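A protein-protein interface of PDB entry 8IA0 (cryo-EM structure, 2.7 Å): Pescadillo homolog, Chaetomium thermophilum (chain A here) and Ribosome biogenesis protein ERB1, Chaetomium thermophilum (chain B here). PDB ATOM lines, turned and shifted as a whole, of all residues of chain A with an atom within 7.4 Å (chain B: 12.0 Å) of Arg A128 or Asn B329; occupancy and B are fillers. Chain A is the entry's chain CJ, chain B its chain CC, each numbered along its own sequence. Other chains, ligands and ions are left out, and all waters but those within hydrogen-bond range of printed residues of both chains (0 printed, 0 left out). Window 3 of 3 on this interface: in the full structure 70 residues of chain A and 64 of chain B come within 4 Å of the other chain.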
ATOM      1  N   LEU A 123      12.847 -16.784  23.634  1.00  0.00           N
ATOM      2  CA  LEU A 123      12.080 -15.906  22.761  1.00  0.00           C
ATOM      3  C   LEU A 123      12.652 -14.493  22.746  1.00  0.00           C
ATOM      4  O   LEU A 123      11.914 -13.519  22.587  1.00  0.00           O
ATOM      5  CB  LEU A 123      10.611 -15.881  23.182  1.00  0.00           C
ATOM      6  CG  LEU A 123       9.952 -17.239  23.427  1.00  0.00           C
ATOM      7  CD1 LEU A 123       8.653 -17.075  24.190  1.00  0.00           C
ATOM      8  CD2 LEU A 123       9.714 -17.963  22.113  1.00  0.00           C
ATOM      9  N   ASN A 124      13.969 -14.368  22.915  1.00  0.00           N
ATOM     10  CA  ASN A 124      14.585 -13.046  22.957  1.00  0.00           C
ATOM     11  C   ASN A 124      14.490 -12.348  21.606  1.00  0.00           C
ATOM     12  O   ASN A 124      14.119 -11.171  21.531  1.00  0.00           O
ATOM     13  CB  ASN A 124      16.043 -13.163  23.401  1.00  0.00           C
ATOM     14  CG  ASN A 124      16.209 -14.037  24.624  1.00  0.00           C
ATOM     15  OD1 ASN A 124      15.627 -13.773  25.673  1.00  0.00           O
ATOM     16  ND2 ASN A 124      17.011 -15.086  24.495  1.00  0.00           N
ATOM     17  N   HIS A 125      14.822 -13.056  20.526  1.00  0.00           N
ATOM     18  CA  HIS A 125      14.780 -12.434  19.209  1.00  0.00           C
ATOM     19  C   HIS A 125      13.349 -12.198  18.744  1.00  0.00           C
ATOM     20  O   HIS A 125      13.089 -11.235  18.016  1.00  0.00           O
ATOM     21  CB  HIS A 125      15.542 -13.285  18.194  1.00  0.00           C
ATOM     22  CG  HIS A 125      15.164 -14.734  18.209  1.00  0.00           C
ATOM     23  ND1 HIS A 125      13.957 -15.193  17.731  1.00  0.00           N
ATOM     24  CD2 HIS A 125      15.837 -15.825  18.643  1.00  0.00           C
ATOM     25  CE1 HIS A 125      13.901 -16.505  17.870  1.00  0.00           C
ATOM     26  NE2 HIS A 125      15.029 -16.914  18.421  1.00  0.00           N
ATOM     27  N   ILE A 126      12.415 -13.059  19.151  1.00  0.00           N
ATOM     28  CA  ILE A 126      11.013 -12.863  18.791  1.00  0.00           C
ATOM     29  C   ILE A 126      10.470 -11.602  19.448  1.00  0.00           C
ATOM     30  O   ILE A 126       9.770 -10.802  18.817  1.00  0.00           O
ATOM     31  CB  ILE A 126      10.183 -14.103  19.170  1.00  0.00           C
ATOM     32  CG1 ILE A 126      10.480 -15.254  18.210  1.00  0.00           C
ATOM     33  CG2 ILE A 126       8.703 -13.781  19.160  1.00  0.00           C
ATOM     34  CD1 ILE A 126       9.783 -16.539  18.572  1.00  0.00           C
ATOM     35  N   ILE A 127      10.786 -11.405  20.729  1.00  0.00           N
ATOM     36  CA  ILE A 127      10.319 -10.216  21.432  1.00  0.00           C
ATOM     37  C   ILE A 127      10.943  -8.960  20.836  1.00  0.00           C
ATOM     38  O   ILE A 127      10.274  -7.932  20.679  1.00  0.00           O
ATOM     39  CB  ILE A 127      10.610 -10.339  22.938  1.00  0.00           C
ATOM     40  CG1 ILE A 127       9.689 -11.378  23.570  1.00  0.00           C
ATOM     41  CG2 ILE A 127      10.420  -9.005  23.635  1.00  0.00           C
ATOM     42  CD1 ILE A 127      10.002 -11.664  25.011  1.00  0.00           C
ATOM     43  N   ARG A 128      12.231  -9.024  20.486  1.00  0.00           N
ATOM     44  CA  ARG A 128      12.915  -7.848  19.959  1.00  0.00           C
ATOM     45  C   ARG A 128      12.322  -7.401  18.628  1.00  0.00           C
ATOM     46  O   ARG A 128      12.127  -6.202  18.402  1.00  0.00           O
ATOM     47  CB  ARG A 128      14.408  -8.138  19.809  1.00  0.00           C
ATOM     48  CG  ARG A 128      15.188  -7.023  19.143  1.00  0.00           C
ATOM     49  CD  ARG A 128      15.487  -5.900  20.117  1.00  0.00           C
ATOM     50  NE  ARG A 128      15.592  -4.611  19.444  1.00  0.00           N
ATOM     51  CZ  ARG A 128      16.729  -3.957  19.255  1.00  0.00           C
ATOM     52  NH1 ARG A 128      17.885  -4.440  19.679  1.00  0.00           N
ATOM     53  NH2 ARG A 128      16.707  -2.786  18.623  1.00  0.00           N
ATOM     54  N   GLU A 129      12.031  -8.345  17.733  1.00  0.00           N
ATOM     55  CA  GLU A 129      11.440  -7.970  16.454  1.00  0.00           C
ATOM     56  C   GLU A 129       9.974  -7.591  16.600  1.00  0.00           C
ATOM     57  O   GLU A 129       9.466  -6.782  15.816  1.00  0.00           O
ATOM     58  CB  GLU A 129      11.588  -9.103  15.437  1.00  0.00           C
ATOM     59  CG  GLU A 129      10.975 -10.419  15.864  1.00  0.00           C
ATOM     60  CD  GLU A 129      10.723 -11.345  14.695  1.00  0.00           C
ATOM     61  OE1 GLU A 129      11.688 -11.977  14.214  1.00  0.00           O
ATOM     62  OE2 GLU A 129       9.561 -11.432  14.247  1.00  0.00           O
ATOM     63  N   ARG A 130       9.282  -8.161  17.587  1.00  0.00           N
ATOM     64  CA  ARG A 130       7.890  -7.804  17.822  1.00  0.00           C
ATOM     65  C   ARG A 130       7.759  -6.446  18.498  1.00  0.00           C
ATOM     66  O   ARG A 130       6.796  -5.719  18.236  1.00  0.00           O
ATOM     67  CB  ARG A 130       7.208  -8.886  18.660  1.00  0.00           C
ATOM     68  CG  ARG A 130       5.716  -8.979  18.443  1.00  0.00           C
ATOM     69  CD  ARG A 130       5.114 -10.125  19.223  1.00  0.00           C
ATOM     70  NE  ARG A 130       3.661 -10.029  19.281  1.00  0.00           N
ATOM     71  CZ  ARG A 130       2.883 -10.849  19.974  1.00  0.00           C
ATOM     72  NH1 ARG A 130       3.387 -11.857  20.668  1.00  0.00           N
ATOM     73  NH2 ARG A 130       1.568 -10.653  19.972  1.00  0.00           N
ATOM     74  N   TYR A 131       8.708  -6.089  19.366  1.00  0.00           N
ATOM     75  CA  TYR A 131       8.762  -4.776  20.009  1.00  0.00           C
ATOM     76  C   TYR A 131      10.131  -4.173  19.729  1.00  0.00           C
ATOM     77  O   TYR A 131      11.067  -4.333  20.530  1.00  0.00           O
ATOM     78  CB  TYR A 131       8.501  -4.876  21.508  1.00  0.00           C
ATOM     79  CG  TYR A 131       7.250  -5.638  21.866  1.00  0.00           C
ATOM     80  CD1 TYR A 131       6.013  -5.233  21.397  1.00  0.00           C
ATOM     81  CD2 TYR A 131       7.304  -6.756  22.682  1.00  0.00           C
ATOM     82  CE1 TYR A 131       4.869  -5.924  21.722  1.00  0.00           C
ATOM     83  CE2 TYR A 131       6.163  -7.452  23.015  1.00  0.00           C
ATOM     84  CZ  TYR A 131       4.947  -7.029  22.533  1.00  0.00           C
ATOM     85  OH  TYR A 131       3.803  -7.720  22.859  1.00  0.00           O
ATOM     86  N   PRO A 132      10.299  -3.474  18.602  1.00  0.00           N
ATOM     87  CA  PRO A 132      11.627  -2.953  18.242  1.00  0.00           C
ATOM     88  C   PRO A 132      12.165  -1.898  19.192  1.00  0.00           C
ATOM     89  O   PRO A 132      13.379  -1.661  19.194  1.00  0.00           O
ATOM     90  CB  PRO A 132      11.404  -2.372  16.841  1.00  0.00           C
ATOM     91  CG  PRO A 132       9.950  -2.073  16.783  1.00  0.00           C
ATOM     92  CD  PRO A 132       9.278  -3.133  17.600  1.00  0.00           C
ATOM     93  N   THR A 133      11.316  -1.258  19.991  1.00  0.00           N
ATOM     94  CA  THR A 133      11.753  -0.248  20.943  1.00  0.00           C
ATOM     95  C   THR A 133      11.075  -0.498  22.279  1.00  0.00           C
ATOM     96  O   THR A 133      10.058  -1.192  22.356  1.00  0.00           O
ATOM     97  CB  THR A 133      11.436   1.174  20.458  1.00  0.00           C
ATOM     98  OG1 THR A 133      10.050   1.268  20.116  1.00  0.00           O
ATOM     99  CG2 THR A 133      12.278   1.530  19.245  1.00  0.00           C
ATOM    100  N   PHE A 134      11.656   0.073  23.339  1.00  0.00           N
ATOM    101  CA  PHE A 134      11.066  -0.066  24.666  1.00  0.00           C
ATOM    102  C   PHE A 134       9.678   0.552  24.735  1.00  0.00           C
ATOM    103  O   PHE A 134       8.853   0.133  25.555  1.00  0.00           O
ATOM    104  CB  PHE A 134      11.974   0.568  25.716  1.00  0.00           C
ATOM    105  CG  PHE A 134      11.643   0.165  27.120  1.00  0.00           C
ATOM    106  CD1 PHE A 134      11.538  -1.170  27.466  1.00  0.00           C
ATOM    107  CD2 PHE A 134      11.432   1.121  28.097  1.00  0.00           C
ATOM    108  CE1 PHE A 134      11.233  -1.542  28.760  1.00  0.00           C
ATOM    109  CE2 PHE A 134      11.126   0.755  29.389  1.00  0.00           C
ATOM    110  CZ  PHE A 134      11.026  -0.578  29.720  1.00  0.00           C
ATOM    111  N   PHE A 233       5.219 -16.330  26.548  1.00  0.00           N
ATOM    112  CA  PHE A 233       5.677 -15.107  25.899  1.00  0.00           C
ATOM    113  C   PHE A 233       5.732 -13.943  26.881  1.00  0.00           C
ATOM    114  O   PHE A 233       6.687 -13.159  26.882  1.00  0.00           O
ATOM    115  CB  PHE A 233       4.765 -14.773  24.719  1.00  0.00           C
ATOM    116  CG  PHE A 233       5.084 -13.469  24.055  1.00  0.00           C
ATOM    117  CD1 PHE A 233       6.122 -13.375  23.150  1.00  0.00           C
ATOM    118  CD2 PHE A 233       4.346 -12.335  24.337  1.00  0.00           C
ATOM    119  CE1 PHE A 233       6.415 -12.176  22.541  1.00  0.00           C
ATOM    120  CE2 PHE A 233       4.638 -11.136  23.734  1.00  0.00           C
ATOM    121  CZ  PHE A 233       5.673 -11.057  22.834  1.00  0.00           C
ATOM    122  N   LEU A 237       8.761 -11.388  28.272  1.00  0.00           N
ATOM    123  CA  LEU A 237       8.637  -9.959  28.004  1.00  0.00           C
ATOM    124  C   LEU A 237       8.768  -9.143  29.284  1.00  0.00           C
ATOM    125  O   LEU A 237       9.528  -8.170  29.338  1.00  0.00           O
ATOM    126  CB  LEU A 237       7.302  -9.673  27.319  1.00  0.00           C
ATOM    127  CG  LEU A 237       6.943  -8.198  27.150  1.00  0.00           C
ATOM    128  CD1 LEU A 237       7.985  -7.486  26.307  1.00  0.00           C
ATOM    129  CD2 LEU A 237       5.562  -8.052  26.536  1.00  0.00           C
ATOM    130  N   TYR B 324      20.259  -9.317  30.521  1.00  0.00           N
ATOM    131  CA  TYR B 324      20.838  -8.270  29.694  1.00  0.00           C
ATOM    132  C   TYR B 324      19.717  -7.421  29.115  1.00  0.00           C
ATOM    133  O   TYR B 324      18.554  -7.830  29.087  1.00  0.00           O
ATOM    134  CB  TYR B 324      21.721  -8.856  28.584  1.00  0.00           C
ATOM    135  CG  TYR B 324      20.968  -9.439  27.409  1.00  0.00           C
ATOM    136  CD1 TYR B 324      20.593 -10.774  27.399  1.00  0.00           C
ATOM    137  CD2 TYR B 324      20.661  -8.667  26.298  1.00  0.00           C
ATOM    138  CE1 TYR B 324      19.914 -11.317  26.328  1.00  0.00           C
ATOM    139  CE2 TYR B 324      19.983  -9.201  25.222  1.00  0.00           C
ATOM    140  CZ  TYR B 324      19.613 -10.527  25.242  1.00  0.00           C
ATOM    141  OH  TYR B 324      18.937 -11.067  24.173  1.00  0.00           O
ATOM    142  N   ASP B 325      20.083  -6.229  28.654  1.00  0.00           N
ATOM    143  CA  ASP B 325      19.113  -5.292  28.105  1.00  0.00           C
ATOM    144  C   ASP B 325      18.839  -5.645  26.649  1.00  0.00           C
ATOM    145  O   ASP B 325      19.747  -5.600  25.811  1.00  0.00           O
ATOM    146  CB  ASP B 325      19.625  -3.861  28.229  1.00  0.00           C
ATOM    147  CG  ASP B 325      18.622  -2.840  27.737  1.00  0.00           C
ATOM    148  OD1 ASP B 325      17.407  -3.111  27.822  1.00  0.00           O
ATOM    149  OD2 ASP B 325      19.049  -1.766  27.266  1.00  0.00           O
ATOM    150  N   LEU B 326      17.588  -6.001  26.351  1.00  0.00           N
ATOM    151  CA  LEU B 326      17.235  -6.410  24.996  1.00  0.00           C
ATOM    152  C   LEU B 326      17.424  -5.270  24.005  1.00  0.00           C
ATOM    153  O   LEU B 326      17.919  -5.479  22.892  1.00  0.00           O
ATOM    154  CB  LEU B 326      15.794  -6.914  24.965  1.00  0.00           C
ATOM    155  CG  LEU B 326      15.438  -7.873  23.830  1.00  0.00           C
ATOM    156  CD1 LEU B 326      16.196  -9.179  23.980  1.00  0.00           C
ATOM    157  CD2 LEU B 326      13.943  -8.121  23.799  1.00  0.00           C
ATOM    158  N   TRP B 327      17.038  -4.059  24.390  1.00  0.00           N
ATOM    159  CA  TRP B 327      17.134  -2.897  23.511  1.00  0.00           C
ATOM    160  C   TRP B 327      18.453  -2.155  23.701  1.00  0.00           C
ATOM    161  O   TRP B 327      18.482  -0.944  23.911  1.00  0.00           O
ATOM    162  CB  TRP B 327      15.948  -1.974  23.752  1.00  0.00           C
ATOM    163  CG  TRP B 327      14.626  -2.652  23.605  1.00  0.00           C
ATOM    164  CD1 TRP B 327      13.838  -2.673  22.494  1.00  0.00           C
ATOM    165  CD2 TRP B 327      13.931  -3.405  24.604  1.00  0.00           C
ATOM    166  NE1 TRP B 327      12.697  -3.394  22.737  1.00  0.00           N
ATOM    167  CE2 TRP B 327      12.729  -3.853  24.026  1.00  0.00           C
ATOM    168  CE3 TRP B 327      14.207  -3.744  25.930  1.00  0.00           C
ATOM    169  CZ2 TRP B 327      11.807  -4.622  24.726  1.00  0.00           C
ATOM    170  CZ3 TRP B 327      13.290  -4.508  26.624  1.00  0.00           C
ATOM    171  CH2 TRP B 327      12.105  -4.937  26.021  1.00  0.00           C
ATOM    172  N   GLN B 328      19.565  -2.887  23.627  1.00  0.00           N
ATOM    173  CA  GLN B 328      20.873  -2.260  23.795  1.00  0.00           C
ATOM    174  C   GLN B 328      21.204  -1.358  22.613  1.00  0.00           C
ATOM    175  O   GLN B 328      21.618  -0.207  22.794  1.00  0.00           O
ATOM    176  CB  GLN B 328      21.948  -3.330  23.979  1.00  0.00           C
ATOM    177  CG  GLN B 328      23.362  -2.779  24.040  1.00  0.00           C
ATOM    178  CD  GLN B 328      23.629  -1.998  25.311  1.00  0.00           C
ATOM    179  OE1 GLN B 328      23.194  -2.389  26.395  1.00  0.00           O
ATOM    180  NE2 GLN B 328      24.346  -0.889  25.185  1.00  0.00           N
ATOM    181  N   ASN B 329      21.026  -1.862  21.397  1.00  0.00           N
ATOM    182  CA  ASN B 329      21.255  -1.099  20.173  1.00  0.00           C
ATOM    183  C   ASN B 329      19.894  -0.902  19.514  1.00  0.00           C
ATOM    184  O   ASN B 329      19.478  -1.685  18.659  1.00  0.00           O
ATOM    185  CB  ASN B 329      22.237  -1.816  19.251  1.00  0.00           C
ATOM    186  CG  ASN B 329      23.645  -1.848  19.813  1.00  0.00           C
ATOM    187  OD1 ASN B 329      24.124  -0.863  20.376  1.00  0.00           O
ATOM    188  ND2 ASN B 329      24.317  -2.983  19.663  1.00  0.00           N
ATOM    189  N   GLU B 330      19.202   0.157  19.922  1.00  0.00           N
ATOM    190  CA  GLU B 330      17.817   0.397  19.548  1.00  0.00           C
ATOM    191  C   GLU B 330      17.698   1.736  18.837  1.00  0.00           C
ATOM    192  O   GLU B 330      18.180   2.756  19.339  1.00  0.00           O
ATOM    193  CB  GLU B 330      16.920   0.369  20.788  1.00  0.00           C
ATOM    194  CG  GLU B 330      15.676   1.229  20.695  1.00  0.00           C
ATOM    195  CD  GLU B 330      15.222   1.723  22.052  1.00  0.00           C
ATOM    196  OE1 GLU B 330      16.093   1.993  22.906  1.00  0.00           O
ATOM    197  OE2 GLU B 330      13.999   1.843  22.269  1.00  0.00           O
ATOM    198  N   GLU B 331      17.060   1.727  17.666  1.00  0.00           N
ATOM    199  CA  GLU B 331      16.764   2.945  16.933  1.00  0.00           C
ATOM    200  C   GLU B 331      15.333   2.867  16.416  1.00  0.00           C
ATOM    201  O   GLU B 331      14.840   1.770  16.112  1.00  0.00           O
ATOM    202  CB  GLU B 331      17.737   3.164  15.765  1.00  0.00           C
ATOM    203  CG  GLU B 331      17.358   2.465  14.469  1.00  0.00           C
ATOM    204  CD  GLU B 331      17.547   0.961  14.537  1.00  0.00           C
ATOM    205  OE1 GLU B 331      18.303   0.493  15.414  1.00  0.00           O
ATOM    206  OE2 GLU B 331      16.939   0.247  13.712  1.00  0.00           O
ATOM    207  N   PRO B 332      14.633   3.999  16.353  1.00  0.00           N
ATOM    208  CA  PRO B 332      13.280   3.995  15.790  1.00  0.00           C
ATOM    209  C   PRO B 332      13.271   3.497  14.352  1.00  0.00           C
ATOM    210  O   PRO B 332      14.200   3.742  13.579  1.00  0.00           O
ATOM    211  CB  PRO B 332      12.864   5.467  15.864  1.00  0.00           C
ATOM    212  CG  PRO B 332      13.660   6.040  16.991  1.00  0.00           C
ATOM    213  CD  PRO B 332      14.850   5.144  17.252  1.00  0.00           C
ATOM    214  N   GLN B 333      12.204   2.789  13.998  1.00  0.00           N
ATOM    215  CA  GLN B 333      12.000   2.298  12.646  1.00  0.00           C
ATOM    216  C   GLN B 333      10.617   2.696  12.153  1.00  0.00           C
ATOM    217  O   GLN B 333       9.688   2.845  12.953  1.00  0.00           O
ATOM    218  CB  GLN B 333      12.153   0.771  12.572  1.00  0.00           C
ATOM    219  CG  GLN B 333      13.000   0.165  13.675  1.00  0.00           C
ATOM    220  CD  GLN B 333      12.727  -1.312  13.871  1.00  0.00           C
ATOM    221  OE1 GLN B 333      11.660  -1.811  13.513  1.00  0.00           O
ATOM    222  NE2 GLN B 333      13.694  -2.022  14.441  1.00  0.00           N
ATOM    223  N   PRO B 334      10.453   2.879  10.845  1.00  0.00           N
ATOM    224  CA  PRO B 334       9.151   3.289  10.308  1.00  0.00           C
ATOM    225  C   PRO B 334       8.127   2.178  10.448  1.00  0.00           C
ATOM    226  O   PRO B 334       8.417   1.011  10.145  1.00  0.00           O
ATOM    227  CB  PRO B 334       9.450   3.586   8.830  1.00  0.00           C
ATOM    228  CG  PRO B 334      10.941   3.701   8.741  1.00  0.00           C
ATOM    229  CD  PRO B 334      11.477   2.792   9.792  1.00  0.00           C
ATOM    230  N   ASN B 336       5.409  -0.308   9.447  1.00  0.00           N
ATOM    231  CA  ASN B 336       4.901  -0.864   8.204  1.00  0.00           C
ATOM    232  C   ASN B 336       3.379  -0.740   8.152  1.00  0.00           C
ATOM    233  O   ASN B 336       2.707  -0.817   9.184  1.00  0.00           O
ATOM    234  CB  ASN B 336       5.308  -2.327   8.065  1.00  0.00           C
ATOM    235  CG  ASN B 336       5.010  -3.136   9.307  1.00  0.00           C
ATOM    236  OD1 ASN B 336       4.592  -2.596  10.330  1.00  0.00           O
ATOM    237  ND2 ASN B 336       5.222  -4.444   9.223  1.00  0.00           N
ATOM    238  N   HIS B 339       0.653  -3.806   9.297  1.00  0.00           N
ATOM    239  CA  HIS B 339       0.364  -4.149  10.680  1.00  0.00           C
ATOM    240  C   HIS B 339      -0.928  -3.477  11.122  1.00  0.00           C
ATOM    241  O   HIS B 339      -1.084  -2.261  10.981  1.00  0.00           O
ATOM    242  CB  HIS B 339       1.516  -3.734  11.593  1.00  0.00           C
ATOM    243  CG  HIS B 339       1.322  -4.129  13.023  1.00  0.00           C
ATOM    244  ND1 HIS B 339       1.300  -5.443  13.436  1.00  0.00           N
ATOM    245  CD2 HIS B 339       1.144  -3.381  14.138  1.00  0.00           C
ATOM    246  CE1 HIS B 339       1.114  -5.489  14.743  1.00  0.00           C
ATOM    247  NE2 HIS B 339       1.017  -4.250  15.193  1.00  0.00           N
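NH1 of Arg A128 is in hydrogen-bond range of O of Leu B326 (3.4 Å).
NH2 of Arg A128 is in hydrogen-bond range of O of Asn B329 (3.0 Å).
O of Tyr A131 sits at hydrogen-bond distance from NE1 of Trp B327.
The backbone carbonyl oxygen of Thr A133 sits close to the indole nitrogen of Trp B327, at 3.5 Å.
The side-chain carboxylate of Glu B330 is in hydrogen-bond range of the backbone NH of Phe A134, 3.1 Å away.
CB of Asn A124 touches OH of Tyr B324, at 3.7 Å.
O of Asn A124 touches CD1 of Leu B326, at 3.8 Å.
Ile A127 touches Leu B326.
Glu B330 touches Arg A128.
Pro A132 touches Trp B327.
Glu B330 touches Pro A132 (CG to O, 3.99 Å).
Gln B333 touches Pro A132.
Thr A133 touches Glu B330 (CB to OE2, 3.2 Å).
CD1 of Trp B327 touches N of Phe A134, at 3.6 Å.
Leu A123 touches none of the printed residues of chain B.
Of the printed residues of chain B, Arg A128 touches Leu B326, Asn B329 and Glu B330.
No residue of chain B comes within 4 Å of Glu A129.
Printed residues of chain A within 4 Å of Tyr B324: Asn A124.
Asn B329 touches just one residue of chain A: Arg A128.
Of the printed residues of chain A, Gln B333 touches Pro A132.
Pro B334 touches none of the printed residues of chain A.
The nearest printed residue of chain B that does not touch Arg A128 is Trp B327 (4.02 Å).
The nearest residue of chain A that does not touch Asn B329 is Pro A132 (6.1 Å).
The nearest printed residue of chain B that does not touch Phe A134 is Asp B325 (6.2 Å).
Of the 14 printed residues of chain A, 7 touch a printed residue of chain B.
Hydrophobic or aromatic side chains of chain A within 4 Å of the printed part of chain B: Ile A127, Pro A132 and Phe A134.
Along chain A the printed residues that touch a printed residue of chain B span positions 124 to 134.
Hydrophobic or aromatic side chains of chain B that line the printed part of chain A: Tyr B324, Leu B326 and Trp B327.
Along chain B the printed residues that touch a printed residue of chain A span positions 324 to 333.
Among the printed residues, 14 pairs touch across the chains.
Among the printed residues, no Asp or Glu carboxylate lies within 4 Å of a Lys or Arg side-chain nitrogen of the other chain.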
